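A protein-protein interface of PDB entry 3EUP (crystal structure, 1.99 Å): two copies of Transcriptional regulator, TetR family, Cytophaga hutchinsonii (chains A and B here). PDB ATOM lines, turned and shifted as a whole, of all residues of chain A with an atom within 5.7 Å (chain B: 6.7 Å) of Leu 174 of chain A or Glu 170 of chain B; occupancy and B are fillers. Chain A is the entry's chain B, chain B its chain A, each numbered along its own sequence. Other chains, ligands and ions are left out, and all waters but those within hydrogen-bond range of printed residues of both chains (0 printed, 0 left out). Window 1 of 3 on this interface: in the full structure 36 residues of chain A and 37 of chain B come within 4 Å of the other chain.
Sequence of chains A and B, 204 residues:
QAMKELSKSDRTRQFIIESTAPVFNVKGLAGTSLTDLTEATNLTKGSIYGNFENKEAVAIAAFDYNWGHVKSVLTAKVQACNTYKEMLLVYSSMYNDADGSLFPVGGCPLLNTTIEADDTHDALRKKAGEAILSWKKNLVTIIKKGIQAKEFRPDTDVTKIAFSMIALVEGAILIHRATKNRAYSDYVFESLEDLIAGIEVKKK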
ATOM      1  N   LEU A 111      -8.947   0.134  25.729  1.00  0.00           N
ATOM      2  CA  LEU A 111      -9.576   1.324  25.186  1.00  0.00           C
ATOM      3  C   LEU A 111      -8.652   2.555  25.187  1.00  0.00           C
ATOM      4  O   LEU A 111      -8.495   3.234  24.139  1.00  0.00           O
ATOM      5  CB  LEU A 111     -10.844   1.601  25.986  1.00  0.00           C
ATOM      6  CG  LEU A 111     -11.910   2.589  25.612  1.00  0.00           C
ATOM      7  CD1 LEU A 111     -12.414   2.374  24.231  1.00  0.00           C
ATOM      8  CD2 LEU A 111     -13.121   2.465  26.623  1.00  0.00           C
ATOM      9  N   ALA A 167     -17.050  -5.640  21.520  1.00  0.00           N
ATOM     10  CA  ALA A 167     -17.558  -4.338  21.072  1.00  0.00           C
ATOM     11  C   ALA A 167     -18.542  -3.789  22.068  1.00  0.00           C
ATOM     12  O   ALA A 167     -18.458  -2.625  22.430  1.00  0.00           O
ATOM     13  CB  ALA A 167     -18.212  -4.442  19.665  1.00  0.00           C
ATOM     14  N   VAL A 169     -18.818  -4.605  25.372  1.00  0.00           N
ATOM     15  CA  VAL A 169     -18.190  -4.299  26.643  1.00  0.00           C
ATOM     16  C   VAL A 169     -17.440  -2.979  26.535  1.00  0.00           C
ATOM     17  O   VAL A 169     -17.604  -2.054  27.386  1.00  0.00           O
ATOM     18  CB  VAL A 169     -17.220  -5.410  27.110  1.00  0.00           C
ATOM     19  CG1 VAL A 169     -16.426  -4.917  28.372  1.00  0.00           C
ATOM     20  CG2 VAL A 169     -17.976  -6.709  27.434  1.00  0.00           C
ATOM     21  N   GLU A 170     -16.606  -2.858  25.490  1.00  0.00           N
ATOM     22  CA  GLU A 170     -15.850  -1.620  25.333  1.00  0.00           C
ATOM     23  C   GLU A 170     -16.761  -0.413  25.038  1.00  0.00           C
ATOM     24  O   GLU A 170     -16.482   0.683  25.493  1.00  0.00           O
ATOM     25  CB  GLU A 170     -14.749  -1.795  24.291  1.00  0.00           C
ATOM     26  CG  GLU A 170     -13.770  -2.939  24.623  1.00  0.00           C
ATOM     27  CD  GLU A 170     -13.043  -2.725  25.963  1.00  0.00           C
ATOM     28  OE1 GLU A 170     -12.221  -1.799  26.088  1.00  0.00           O
ATOM     29  OE2 GLU A 170     -13.314  -3.476  26.899  1.00  0.00           O
ATOM     30  N   GLY A 171     -17.830  -0.614  24.276  1.00  0.00           N
ATOM     31  CA  GLY A 171     -18.765   0.441  23.972  1.00  0.00           C
ATOM     32  C   GLY A 171     -19.529   0.851  25.203  1.00  0.00           C
ATOM     33  O   GLY A 171     -19.813   2.022  25.406  1.00  0.00           O
ATOM     34  N   ALA A 172     -19.878  -0.122  26.050  1.00  0.00           N
ATOM     35  CA  ALA A 172     -20.528   0.181  27.317  1.00  0.00           C
ATOM     36  C   ALA A 172     -19.605   1.076  28.174  1.00  0.00           C
ATOM     37  O   ALA A 172     -20.027   2.077  28.734  1.00  0.00           O
ATOM     38  CB  ALA A 172     -20.933  -1.131  28.078  1.00  0.00           C
ATOM     39  N   ILE A 173     -18.335   0.708  28.254  1.00  0.00           N
ATOM     40  CA  ILE A 173     -17.367   1.499  29.033  1.00  0.00           C
ATOM     41  C   ILE A 173     -17.283   2.951  28.482  1.00  0.00           C
ATOM     42  O   ILE A 173     -17.299   3.932  29.259  1.00  0.00           O
ATOM     43  CB  ILE A 173     -15.991   0.761  29.069  1.00  0.00           C
ATOM     44  CG1 ILE A 173     -16.083  -0.524  29.925  1.00  0.00           C
ATOM     45  CG2 ILE A 173     -14.945   1.667  29.601  1.00  0.00           C
ATOM     46  CD1 ILE A 173     -14.796  -1.439  29.892  1.00  0.00           C
ATOM     47  N   LEU A 174     -17.206   3.081  27.150  1.00  0.00           N
ATOM     48  CA  LEU A 174     -17.178   4.386  26.520  1.00  0.00           C
ATOM     49  C   LEU A 174     -18.354   5.236  26.945  1.00  0.00           C
ATOM     50  O   LEU A 174     -18.189   6.398  27.300  1.00  0.00           O
ATOM     51  CB  LEU A 174     -17.163   4.264  24.980  1.00  0.00           C
ATOM     52  CG  LEU A 174     -17.209   5.572  24.183  1.00  0.00           C
ATOM     53  CD1 LEU A 174     -16.016   6.431  24.473  1.00  0.00           C
ATOM     54  CD2 LEU A 174     -17.227   5.265  22.734  1.00  0.00           C
ATOM     55  N   ILE A 175     -19.539   4.659  26.881  1.00  0.00           N
ATOM     56  CA  ILE A 175     -20.763   5.396  27.192  1.00  0.00           C
ATOM     57  C   ILE A 175     -20.717   5.858  28.657  1.00  0.00           C
ATOM     58  O   ILE A 175     -21.008   7.039  28.951  1.00  0.00           O
ATOM     59  CB  ILE A 175     -22.029   4.563  26.861  1.00  0.00           C
ATOM     60  CG1 ILE A 175     -22.191   4.460  25.334  1.00  0.00           C
ATOM     61  CG2 ILE A 175     -23.306   5.149  27.575  1.00  0.00           C
ATOM     62  CD1 ILE A 175     -23.066   3.265  24.892  1.00  0.00           C
ATOM     63  N   HIS A 176     -20.306   4.949  29.566  1.00  0.00           N
ATOM     64  CA  HIS A 176     -20.141   5.306  30.964  1.00  0.00           C
ATOM     65  C   HIS A 176     -19.133   6.430  31.177  1.00  0.00           C
ATOM     66  O   HIS A 176     -19.377   7.379  31.945  1.00  0.00           O
ATOM     67  CB  HIS A 176     -19.708   4.125  31.826  1.00  0.00           C
ATOM     68  CG  HIS A 176     -19.338   4.535  33.202  1.00  0.00           C
ATOM     69  ND1 HIS A 176     -20.244   5.116  34.062  1.00  0.00           N
ATOM     70  CD2 HIS A 176     -18.159   4.523  33.854  1.00  0.00           C
ATOM     71  CE1 HIS A 176     -19.644   5.426  35.196  1.00  0.00           C
ATOM     72  NE2 HIS A 176     -18.377   5.076  35.099  1.00  0.00           N
ATOM     73  N   ARG A 177     -18.003   6.358  30.502  1.00  0.00           N
ATOM     74  CA  ARG A 177     -16.994   7.390  30.723  1.00  0.00           C
ATOM     75  C   ARG A 177     -17.347   8.752  30.110  1.00  0.00           C
ATOM     76  O   ARG A 177     -16.940   9.777  30.663  1.00  0.00           O
ATOM     77  CB  ARG A 177     -15.646   6.872  30.292  1.00  0.00           C
ATOM     78  CG  ARG A 177     -15.358   5.561  31.118  1.00  0.00           C
ATOM     79  CD  ARG A 177     -13.926   5.162  31.058  1.00  0.00           C
ATOM     80  NE  ARG A 177     -13.128   5.819  32.087  1.00  0.00           N
ATOM     81  CZ  ARG A 177     -12.967   5.361  33.336  1.00  0.00           C
ATOM     82  NH1 ARG A 177     -12.156   6.010  34.184  1.00  0.00           N
ATOM     83  NH2 ARG A 177     -13.614   4.264  33.744  1.00  0.00           N
ATOM     84  N   ALA A 178     -18.142   8.743  29.043  1.00  0.00           N
ATOM     85  CA  ALA A 178     -18.567   9.968  28.369  1.00  0.00           C
ATOM     86  C   ALA A 178     -19.685  10.602  29.204  1.00  0.00           C
ATOM     87  O   ALA A 178     -19.737  11.810  29.292  1.00  0.00           O
ATOM     88  CB  ALA A 178     -19.074   9.693  26.989  1.00  0.00           C
ATOM     89  N   THR A 179     -20.577   9.801  29.773  1.00  0.00           N
ATOM     90  CA  THR A 179     -21.763  10.363  30.480  1.00  0.00           C
ATOM     91  C   THR A 179     -21.702  10.384  31.997  1.00  0.00           C
ATOM     92  O   THR A 179     -22.544  11.034  32.612  1.00  0.00           O
ATOM     93  CB  THR A 179     -23.013   9.567  30.136  1.00  0.00           C
ATOM     94  OG1 THR A 179     -22.859   8.204  30.603  1.00  0.00           O
ATOM     95  CG2 THR A 179     -23.311   9.649  28.578  1.00  0.00           C
ATOM     96  N   TRP B  67     -16.898  16.355  15.305  1.00  0.00           N
ATOM     97  CA  TRP B  67     -18.151  15.708  15.558  1.00  0.00           C
ATOM     98  C   TRP B  67     -19.265  16.311  14.686  1.00  0.00           C
ATOM     99  O   TRP B  67     -20.109  15.579  14.193  1.00  0.00           O
ATOM    100  CB  TRP B  67     -18.481  15.751  17.046  1.00  0.00           C
ATOM    101  CG  TRP B  67     -19.718  15.011  17.363  1.00  0.00           C
ATOM    102  CD1 TRP B  67     -20.905  15.541  17.771  1.00  0.00           C
ATOM    103  CD2 TRP B  67     -19.937  13.607  17.199  1.00  0.00           C
ATOM    104  NE1 TRP B  67     -21.825  14.542  17.939  1.00  0.00           N
ATOM    105  CE2 TRP B  67     -21.257  13.348  17.581  1.00  0.00           C
ATOM    106  CE3 TRP B  67     -19.121  12.538  16.803  1.00  0.00           C
ATOM    107  CZ2 TRP B  67     -21.784  12.067  17.596  1.00  0.00           C
ATOM    108  CZ3 TRP B  67     -19.644  11.264  16.817  1.00  0.00           C
ATOM    109  CH2 TRP B  67     -20.960  11.039  17.214  1.00  0.00           C
ATOM    110  N   PHE B 103     -14.977   9.877   7.582  1.00  0.00           N
ATOM    111  CA  PHE B 103     -14.736  10.238   8.980  1.00  0.00           C
ATOM    112  C   PHE B 103     -13.569  11.192   9.087  1.00  0.00           C
ATOM    113  O   PHE B 103     -12.687  11.193   8.222  1.00  0.00           O
ATOM    114  CB  PHE B 103     -14.386   9.013   9.823  1.00  0.00           C
ATOM    115  CG  PHE B 103     -15.517   8.515  10.675  1.00  0.00           C
ATOM    116  CD1 PHE B 103     -16.575   7.870  10.106  1.00  0.00           C
ATOM    117  CD2 PHE B 103     -15.487   8.653  12.047  1.00  0.00           C
ATOM    118  CE1 PHE B 103     -17.603   7.392  10.889  1.00  0.00           C
ATOM    119  CE2 PHE B 103     -16.524   8.198  12.820  1.00  0.00           C
ATOM    120  CZ  PHE B 103     -17.573   7.567  12.235  1.00  0.00           C
ATOM    121  N   CYS B 108     -13.039   8.491  15.212  1.00  0.00           N
ATOM    122  CA  CYS B 108     -14.205   9.045  15.860  1.00  0.00           C
ATOM    123  C   CYS B 108     -13.778  10.013  16.943  1.00  0.00           C
ATOM    124  O   CYS B 108     -13.092   9.613  17.886  1.00  0.00           O
ATOM    125  CB  CYS B 108     -15.078   7.966  16.492  1.00  0.00           C
ATOM    126  SG  CYS B 108     -16.561   8.614  17.277  1.00  0.00           S
ATOM    127  N   PRO B 109     -14.181  11.297  16.812  1.00  0.00           N
ATOM    128  CA  PRO B 109     -13.825  12.253  17.859  1.00  0.00           C
ATOM    129  C   PRO B 109     -14.494  11.972  19.214  1.00  0.00           C
ATOM    130  O   PRO B 109     -13.991  12.406  20.264  1.00  0.00           O
ATOM    131  CB  PRO B 109     -14.267  13.591  17.291  1.00  0.00           C
ATOM    132  CG  PRO B 109     -15.286  13.272  16.233  1.00  0.00           C
ATOM    133  CD  PRO B 109     -14.896  11.924  15.684  1.00  0.00           C
ATOM    134  N   LEU B 110     -15.623  11.263  19.202  1.00  0.00           N
ATOM    135  CA  LEU B 110     -16.347  11.032  20.431  1.00  0.00           C
ATOM    136  C   LEU B 110     -15.565  10.008  21.247  1.00  0.00           C
ATOM    137  O   LEU B 110     -15.284  10.207  22.442  1.00  0.00           O
ATOM    138  CB  LEU B 110     -17.769  10.591  20.092  1.00  0.00           C
ATOM    139  CG  LEU B 110     -18.710  10.088  21.148  1.00  0.00           C
ATOM    140  CD1 LEU B 110     -20.109   9.914  20.512  1.00  0.00           C
ATOM    141  CD2 LEU B 110     -18.165   8.793  21.714  1.00  0.00           C
ATOM    142  N   LEU B 111     -15.153   8.941  20.561  1.00  0.00           N
ATOM    143  CA  LEU B 111     -14.283   7.966  21.159  1.00  0.00           C
ATOM    144  C   LEU B 111     -12.975   8.617  21.572  1.00  0.00           C
ATOM    145  O   LEU B 111     -12.562   8.470  22.677  1.00  0.00           O
ATOM    146  CB  LEU B 111     -14.085   6.879  20.109  1.00  0.00           C
ATOM    147  CG  LEU B 111     -13.440   5.578  20.378  1.00  0.00           C
ATOM    148  CD1 LEU B 111     -14.100   4.809  21.550  1.00  0.00           C
ATOM    149  CD2 LEU B 111     -13.510   4.761  19.041  1.00  0.00           C
ATOM    150  N   ASN B 112     -12.343   9.399  20.700  1.00  0.00           N
ATOM    151  CA  ASN B 112     -11.034   9.924  20.966  1.00  0.00           C
ATOM    152  C   ASN B 112     -11.043  10.950  22.064  1.00  0.00           C
ATOM    153  O   ASN B 112     -10.100  11.014  22.907  1.00  0.00           O
ATOM    154  CB  ASN B 112     -10.410  10.554  19.712  1.00  0.00           C
ATOM    155  CG  ASN B 112     -10.280   9.570  18.566  1.00  0.00           C
ATOM    156  OD1 ASN B 112     -10.472   8.348  18.734  1.00  0.00           O
ATOM    157  ND2 ASN B 112     -10.036  10.105  17.365  1.00  0.00           N
ATOM    158  N   THR B 114     -13.437  11.297  24.528  1.00  0.00           N
ATOM    159  CA  THR B 114     -13.861  10.722  25.783  1.00  0.00           C
ATOM    160  C   THR B 114     -12.659  10.085  26.523  1.00  0.00           C
ATOM    161  O   THR B 114     -12.521  10.264  27.724  1.00  0.00           O
ATOM    162  CB  THR B 114     -14.964   9.610  25.601  1.00  0.00           C
ATOM    163  OG1 THR B 114     -16.121  10.173  24.987  1.00  0.00           O
ATOM    164  CG2 THR B 114     -15.374   9.007  26.975  1.00  0.00           C
ATOM    165  N   ILE B 115     -11.811   9.333  25.829  1.00  0.00           N
ATOM    166  CA  ILE B 115     -10.724   8.616  26.478  1.00  0.00           C
ATOM    167  C   ILE B 115      -9.722   9.603  27.078  1.00  0.00           C
ATOM    168  O   ILE B 115      -9.184   9.400  28.185  1.00  0.00           O
ATOM    169  CB  ILE B 115     -10.039   7.662  25.444  1.00  0.00           C
ATOM    170  CG1 ILE B 115     -11.076   6.718  24.865  1.00  0.00           C
ATOM    171  CG2 ILE B 115      -8.925   6.846  26.101  1.00  0.00           C
ATOM    172  CD1 ILE B 115     -11.781   5.859  25.878  1.00  0.00           C
ATOM    173  N   ILE B 132     -23.086  12.134  22.880  1.00  0.00           N
ATOM    174  CA  ILE B 132     -23.566  10.784  22.954  1.00  0.00           C
ATOM    175  C   ILE B 132     -25.048  10.815  23.207  1.00  0.00           C
ATOM    176  O   ILE B 132     -25.777  10.046  22.626  1.00  0.00           O
ATOM    177  CB  ILE B 132     -22.877  10.038  24.150  1.00  0.00           C
ATOM    178  CG1 ILE B 132     -21.531   9.532  23.746  1.00  0.00           C
ATOM    179  CG2 ILE B 132     -23.765   8.878  24.721  1.00  0.00           C
ATOM    180  CD1 ILE B 132     -21.603   8.101  23.086  1.00  0.00           C
ATOM    181  N   TRP B 135     -26.999  11.973  20.068  1.00  0.00           N
ATOM    182  CA  TRP B 135     -26.982  10.885  19.123  1.00  0.00           C
ATOM    183  C   TRP B 135     -28.039   9.883  19.563  1.00  0.00           C
ATOM    184  O   TRP B 135     -28.900   9.532  18.754  1.00  0.00           O
ATOM    185  CB  TRP B 135     -25.599  10.252  19.040  1.00  0.00           C
ATOM    186  CG  TRP B 135     -25.437   9.145  18.073  1.00  0.00           C
ATOM    187  CD1 TRP B 135     -26.304   8.736  17.101  1.00  0.00           C
ATOM    188  CD2 TRP B 135     -24.290   8.291  17.973  1.00  0.00           C
ATOM    189  NE1 TRP B 135     -25.773   7.663  16.420  1.00  0.00           N
ATOM    190  CE2 TRP B 135     -24.529   7.383  16.936  1.00  0.00           C
ATOM    191  CE3 TRP B 135     -23.085   8.208  18.676  1.00  0.00           C
ATOM    192  CZ2 TRP B 135     -23.594   6.393  16.574  1.00  0.00           C
ATOM    193  CZ3 TRP B 135     -22.133   7.237  18.284  1.00  0.00           C
ATOM    194  CH2 TRP B 135     -22.414   6.341  17.270  1.00  0.00           C
ATOM    195  N   MET B 165     -26.744   0.260  20.033  1.00  0.00           N
ATOM    196  CA  MET B 165     -26.292   0.623  18.682  1.00  0.00           C
ATOM    197  C   MET B 165     -25.017   1.430  18.796  1.00  0.00           C
ATOM    198  O   MET B 165     -24.036   1.149  18.105  1.00  0.00           O
ATOM    199  CB  MET B 165     -27.359   1.480  17.926  1.00  0.00           C
ATOM    200  CG  MET B 165     -28.650   0.744  17.443  1.00  0.00           C
ATOM    201  SD  MET B 165     -29.892   1.867  16.648  1.00  0.00           S
ATOM    202  CE  MET B 165     -28.847   2.435  15.286  1.00  0.00           C
ATOM    203  N   ILE B 166     -25.059   2.445  19.659  1.00  0.00           N
ATOM    204  CA  ILE B 166     -23.929   3.312  19.928  1.00  0.00           C
ATOM    205  C   ILE B 166     -22.741   2.514  20.397  1.00  0.00           C
ATOM    206  O   ILE B 166     -21.643   2.664  19.882  1.00  0.00           O
ATOM    207  CB  ILE B 166     -24.320   4.430  20.916  1.00  0.00           C
ATOM    208  CG1 ILE B 166     -25.288   5.401  20.202  1.00  0.00           C
ATOM    209  CG2 ILE B 166     -23.045   5.155  21.455  1.00  0.00           C
ATOM    210  CD1 ILE B 166     -25.975   6.472  21.095  1.00  0.00           C
ATOM    211  N   ALA B 167     -22.974   1.585  21.314  1.00  0.00           N
ATOM    212  CA  ALA B 167     -21.920   0.725  21.787  1.00  0.00           C
ATOM    213  C   ALA B 167     -21.339  -0.087  20.665  1.00  0.00           C
ATOM    214  O   ALA B 167     -20.122  -0.246  20.561  1.00  0.00           O
ATOM    215  CB  ALA B 167     -22.426  -0.197  22.922  1.00  0.00           C
ATOM    216  N   LEU B 168     -22.205  -0.653  19.843  1.00  0.00           N
ATOM    217  CA  LEU B 168     -21.739  -1.490  18.774  1.00  0.00           C
ATOM    218  C   LEU B 168     -20.930  -0.730  17.723  1.00  0.00           C
ATOM    219  O   LEU B 168     -19.936  -1.261  17.225  1.00  0.00           O
ATOM    220  CB  LEU B 168     -22.895  -2.224  18.121  1.00  0.00           C
ATOM    221  CG  LEU B 168     -23.467  -3.430  18.871  1.00  0.00           C
ATOM    222  CD1 LEU B 168     -24.781  -3.897  18.154  1.00  0.00           C
ATOM    223  CD2 LEU B 168     -22.422  -4.531  18.967  1.00  0.00           C
ATOM    224  N   VAL B 169     -21.341   0.494  17.384  1.00  0.00           N
ATOM    225  CA  VAL B 169     -20.638   1.275  16.408  1.00  0.00           C
ATOM    226  C   VAL B 169     -19.257   1.702  16.951  1.00  0.00           C
ATOM    227  O   VAL B 169     -18.242   1.481  16.309  1.00  0.00           O
ATOM    228  CB  VAL B 169     -21.467   2.487  15.947  1.00  0.00           C
ATOM    229  CG1 VAL B 169     -20.618   3.441  15.078  1.00  0.00           C
ATOM    230  CG2 VAL B 169     -22.711   1.990  15.164  1.00  0.00           C
ATOM    231  N   GLU B 170     -19.234   2.247  18.167  1.00  0.00           N
ATOM    232  CA  GLU B 170     -18.009   2.707  18.759  1.00  0.00           C
ATOM    233  C   GLU B 170     -17.049   1.550  19.053  1.00  0.00           C
ATOM    234  O   GLU B 170     -15.866   1.704  18.882  1.00  0.00           O
ATOM    235  CB  GLU B 170     -18.307   3.543  19.996  1.00  0.00           C
ATOM    236  CG  GLU B 170     -19.156   4.776  19.674  1.00  0.00           C
ATOM    237  CD  GLU B 170     -18.512   5.682  18.634  1.00  0.00           C
ATOM    238  OE1 GLU B 170     -17.581   6.462  18.993  1.00  0.00           O
ATOM    239  OE2 GLU B 170     -18.971   5.639  17.468  1.00  0.00           O
ATOM    240  N   GLY B 171     -17.590   0.402  19.464  1.00  0.00           N
ATOM    241  CA  GLY B 171     -16.826  -0.814  19.691  1.00  0.00           C
ATOM    242  C   GLY B 171     -16.246  -1.381  18.407  1.00  0.00           C
ATOM    243  O   GLY B 171     -15.106  -1.857  18.417  1.00  0.00           O
ATOM    244  N   ALA B 172     -17.004  -1.295  17.305  1.00  0.00           N
ATOM    245  CA  ALA B 172     -16.523  -1.706  15.988  1.00  0.00           C
ATOM    246  C   ALA B 172     -15.330  -0.855  15.605  1.00  0.00           C
ATOM    247  O   ALA B 172     -14.317  -1.391  15.211  1.00  0.00           O
ATOM    248  CB  ALA B 172     -17.675  -1.640  14.885  1.00  0.00           C
ATOM    249  N   ILE B 173     -15.432   0.468  15.775  1.00  0.00           N
ATOM    250  CA  ILE B 173     -14.342   1.390  15.443  1.00  0.00           C
ATOM    251  C   ILE B 173     -13.083   1.054  16.252  1.00  0.00           C
ATOM    252  O   ILE B 173     -11.966   0.956  15.694  1.00  0.00           O
ATOM    253  CB  ILE B 173     -14.761   2.871  15.564  1.00  0.00           C
ATOM    254  CG1 ILE B 173     -15.896   3.206  14.532  1.00  0.00           C
ATOM    255  CG2 ILE B 173     -13.503   3.819  15.504  1.00  0.00           C
ATOM    256  CD1 ILE B 173     -16.477   4.635  14.634  1.00  0.00           C
ATOM    257  N   LEU B 174     -13.272   0.786  17.540  1.00  0.00           N
ATOM    258  CA  LEU B 174     -12.171   0.458  18.449  1.00  0.00           C
ATOM    259  C   LEU B 174     -11.389  -0.756  17.996  1.00  0.00           C
ATOM    260  O   LEU B 174     -10.166  -0.731  17.963  1.00  0.00           O
ATOM    261  CB  LEU B 174     -12.678   0.227  19.876  1.00  0.00           C
ATOM    262  CG  LEU B 174     -11.580  -0.193  20.863  1.00  0.00           C
ATOM    263  CD1 LEU B 174     -10.628   0.958  21.088  1.00  0.00           C
ATOM    264  CD2 LEU B 174     -12.201  -0.683  22.199  1.00  0.00           C
ATOM    265  N   ILE B 175     -12.109  -1.801  17.611  1.00  0.00           N
ATOM    266  CA  ILE B 175     -11.501  -3.021  17.129  1.00  0.00           C
ATOM    267  C   ILE B 175     -10.756  -2.765  15.819  1.00  0.00           C
ATOM    268  O   ILE B 175      -9.591  -3.203  15.600  1.00  0.00           O
ATOM    269  CB  ILE B 175     -12.565  -4.073  16.949  1.00  0.00           C
ATOM    270  CG1 ILE B 175     -13.072  -4.527  18.322  1.00  0.00           C
ATOM    271  CG2 ILE B 175     -12.055  -5.289  16.110  1.00  0.00           C
ATOM    272  CD1 ILE B 175     -14.370  -5.377  18.294  1.00  0.00           C
ATOM    273  N   PHE B 189     -20.464  -4.830  12.837  1.00  0.00           N
ATOM    274  CA  PHE B 189     -21.489  -4.189  12.023  1.00  0.00           C
ATOM    275  C   PHE B 189     -22.556  -5.204  11.639  1.00  0.00           C
ATOM    276  O   PHE B 189     -23.750  -4.853  11.513  1.00  0.00           O
ATOM    277  CB  PHE B 189     -20.844  -3.522  10.788  1.00  0.00           C
ATOM    278  CG  PHE B 189     -20.131  -2.250  11.128  1.00  0.00           C
ATOM    279  CD1 PHE B 189     -20.858  -1.168  11.610  1.00  0.00           C
ATOM    280  CD2 PHE B 189     -18.771  -2.113  11.005  1.00  0.00           C
ATOM    281  CE1 PHE B 189     -20.235   0.010  11.975  1.00  0.00           C
ATOM    282  CE2 PHE B 189     -18.149  -0.932  11.341  1.00  0.00           C
ATOM    283  CZ  PHE B 189     -18.907   0.154  11.836  1.00  0.00           C
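O of Ala 167 of chain B lies close to O of Ala 167 of chain A (3.5 Å).
OG1 of Thr 114 of chain B lies within hydrogen-bond range of O of Leu 110 of chain B (2.7 Å). O of Ile 175 of chain A lies within hydrogen-bond range of OG1 of Thr 179 of chain A (2.7 Å). The side-chain sulfur of Cys 108 of chain B lies within hydrogen-bond range of the backbone NH of Leu 111 of chain B (3.6 Å). The side-chain sulfur (SG) of Cys 108 of chain B lies close to the backbone NH (N) of Leu 110 of chain B (3.4 Å). OE1 of Glu 170 of chain B lies within hydrogen-bond range of SG of Cys 108 of chain B, at 2.9 Å.
CD1 of Leu 111 of chain B touches CD1 of Leu 111 of chain A (3.99 Å). CD1 of Ile 115 of chain B touches CG of Leu 111 of chain A (3.3 Å). CD2 of Leu 174 of chain B touches CD1 of Leu 111 of chain A, 3.7 Å away. Ala 167 of chain A touches Gly 171 of chain B (O to CA, 3.7 Å). Leu 174 of chain B touches Glu 170 of chain A (CD2 to CB, 3.5 Å). Gly 171 of chain A touches Ala 167 of chain B (CA to O, 3.7 Å). CD2 of Leu 174 of chain A touches CD2 of Leu 110 of chain B, 3.8 Å away. Glu 170 of chain B touches Leu 174 of chain A (CB to CD2, 3.4 Å). Ile 166 of chain B touches Ile 175 of chain A (CG2 to CD1, 3.9 Å). N of Ala 167 of chain B touches CD1 of Ile 175 of chain A, 3.95 Å away.
Leu 174 of chain A touches four residues of chain B. Printed residues of chain A within 4 Å of Glu 170 of chain B: Leu 174. Printed residues of chain A within 4 Å of Ile 166 of chain B: Ile 175 (3.9 Å). Of the printed residues of chain B, Thr 179 of chain A touches Ile 132 (3.96 Å). Printed residues of chain A within 4 Å of Thr 114 of chain B: Leu 174 (3.5 Å), Arg 177 (3.7 Å) and Ala 178 (3.5 Å). Of the printed residues of chain A, Leu 110 of chain B touches Leu 174. The nearest residue of chain B that does not touch Leu 174 of chain A is Ile 115 of chain B (4.5 Å). The nearest residue of chain A that does not touch Glu 170 of chain B is Gly 171 of chain A (5.1 Å).
Printed residues of chain B that touch a printed residue of chain A: Leu 110, Leu 111, Thr 114, Ile 115, Ile 132, Ile 166, Ala 167, Glu 170, Gly 171 and Leu 174. Of the 13 printed residues of chain A, 9 touch a printed residue of chain B. Printed residues of chain A that touch a printed residue of chain B: Leu 111, Ala 167, Glu 170, Gly 171, Leu 174, Ile 175, Arg 177, Ala 178 and Thr 179. Hydrophobic or aromatic side chains of chain A that line the printed part of chain B: Leu 111, Ala 167, Leu 174, Ile 175 and Ala 178. Among the printed residues, 16 pairs touch across the chains. Among the printed residues, no Asp or Glu carboxylate lies within 4 Å of a Lys or Arg side-chain nitrogen of the other chain.
Leu 111 of chain A touches its own counterpart, Leu 111 of chain B. Ala 167 of chain A touches its own counterpart, Ala 167 of chain B. Glu 170 of chain A touches Leu 174 of chain B, and with the chains exchanged Leu 174 of chain A touches Glu 170 of chain B. Ile 175 of chain A touches Ala 167 of chain B, but with the chains exchanged Ala 167 of chain A does not touch Ile 175 of chain B (4.2 Å). Positions printed for both chains: 111, 167, 169, 170, 171, 172, 173, 174 and 175. Of the 16 pairs that touch across the chains among the printed residues, 8 have their exchanged pair printed and touching as well.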
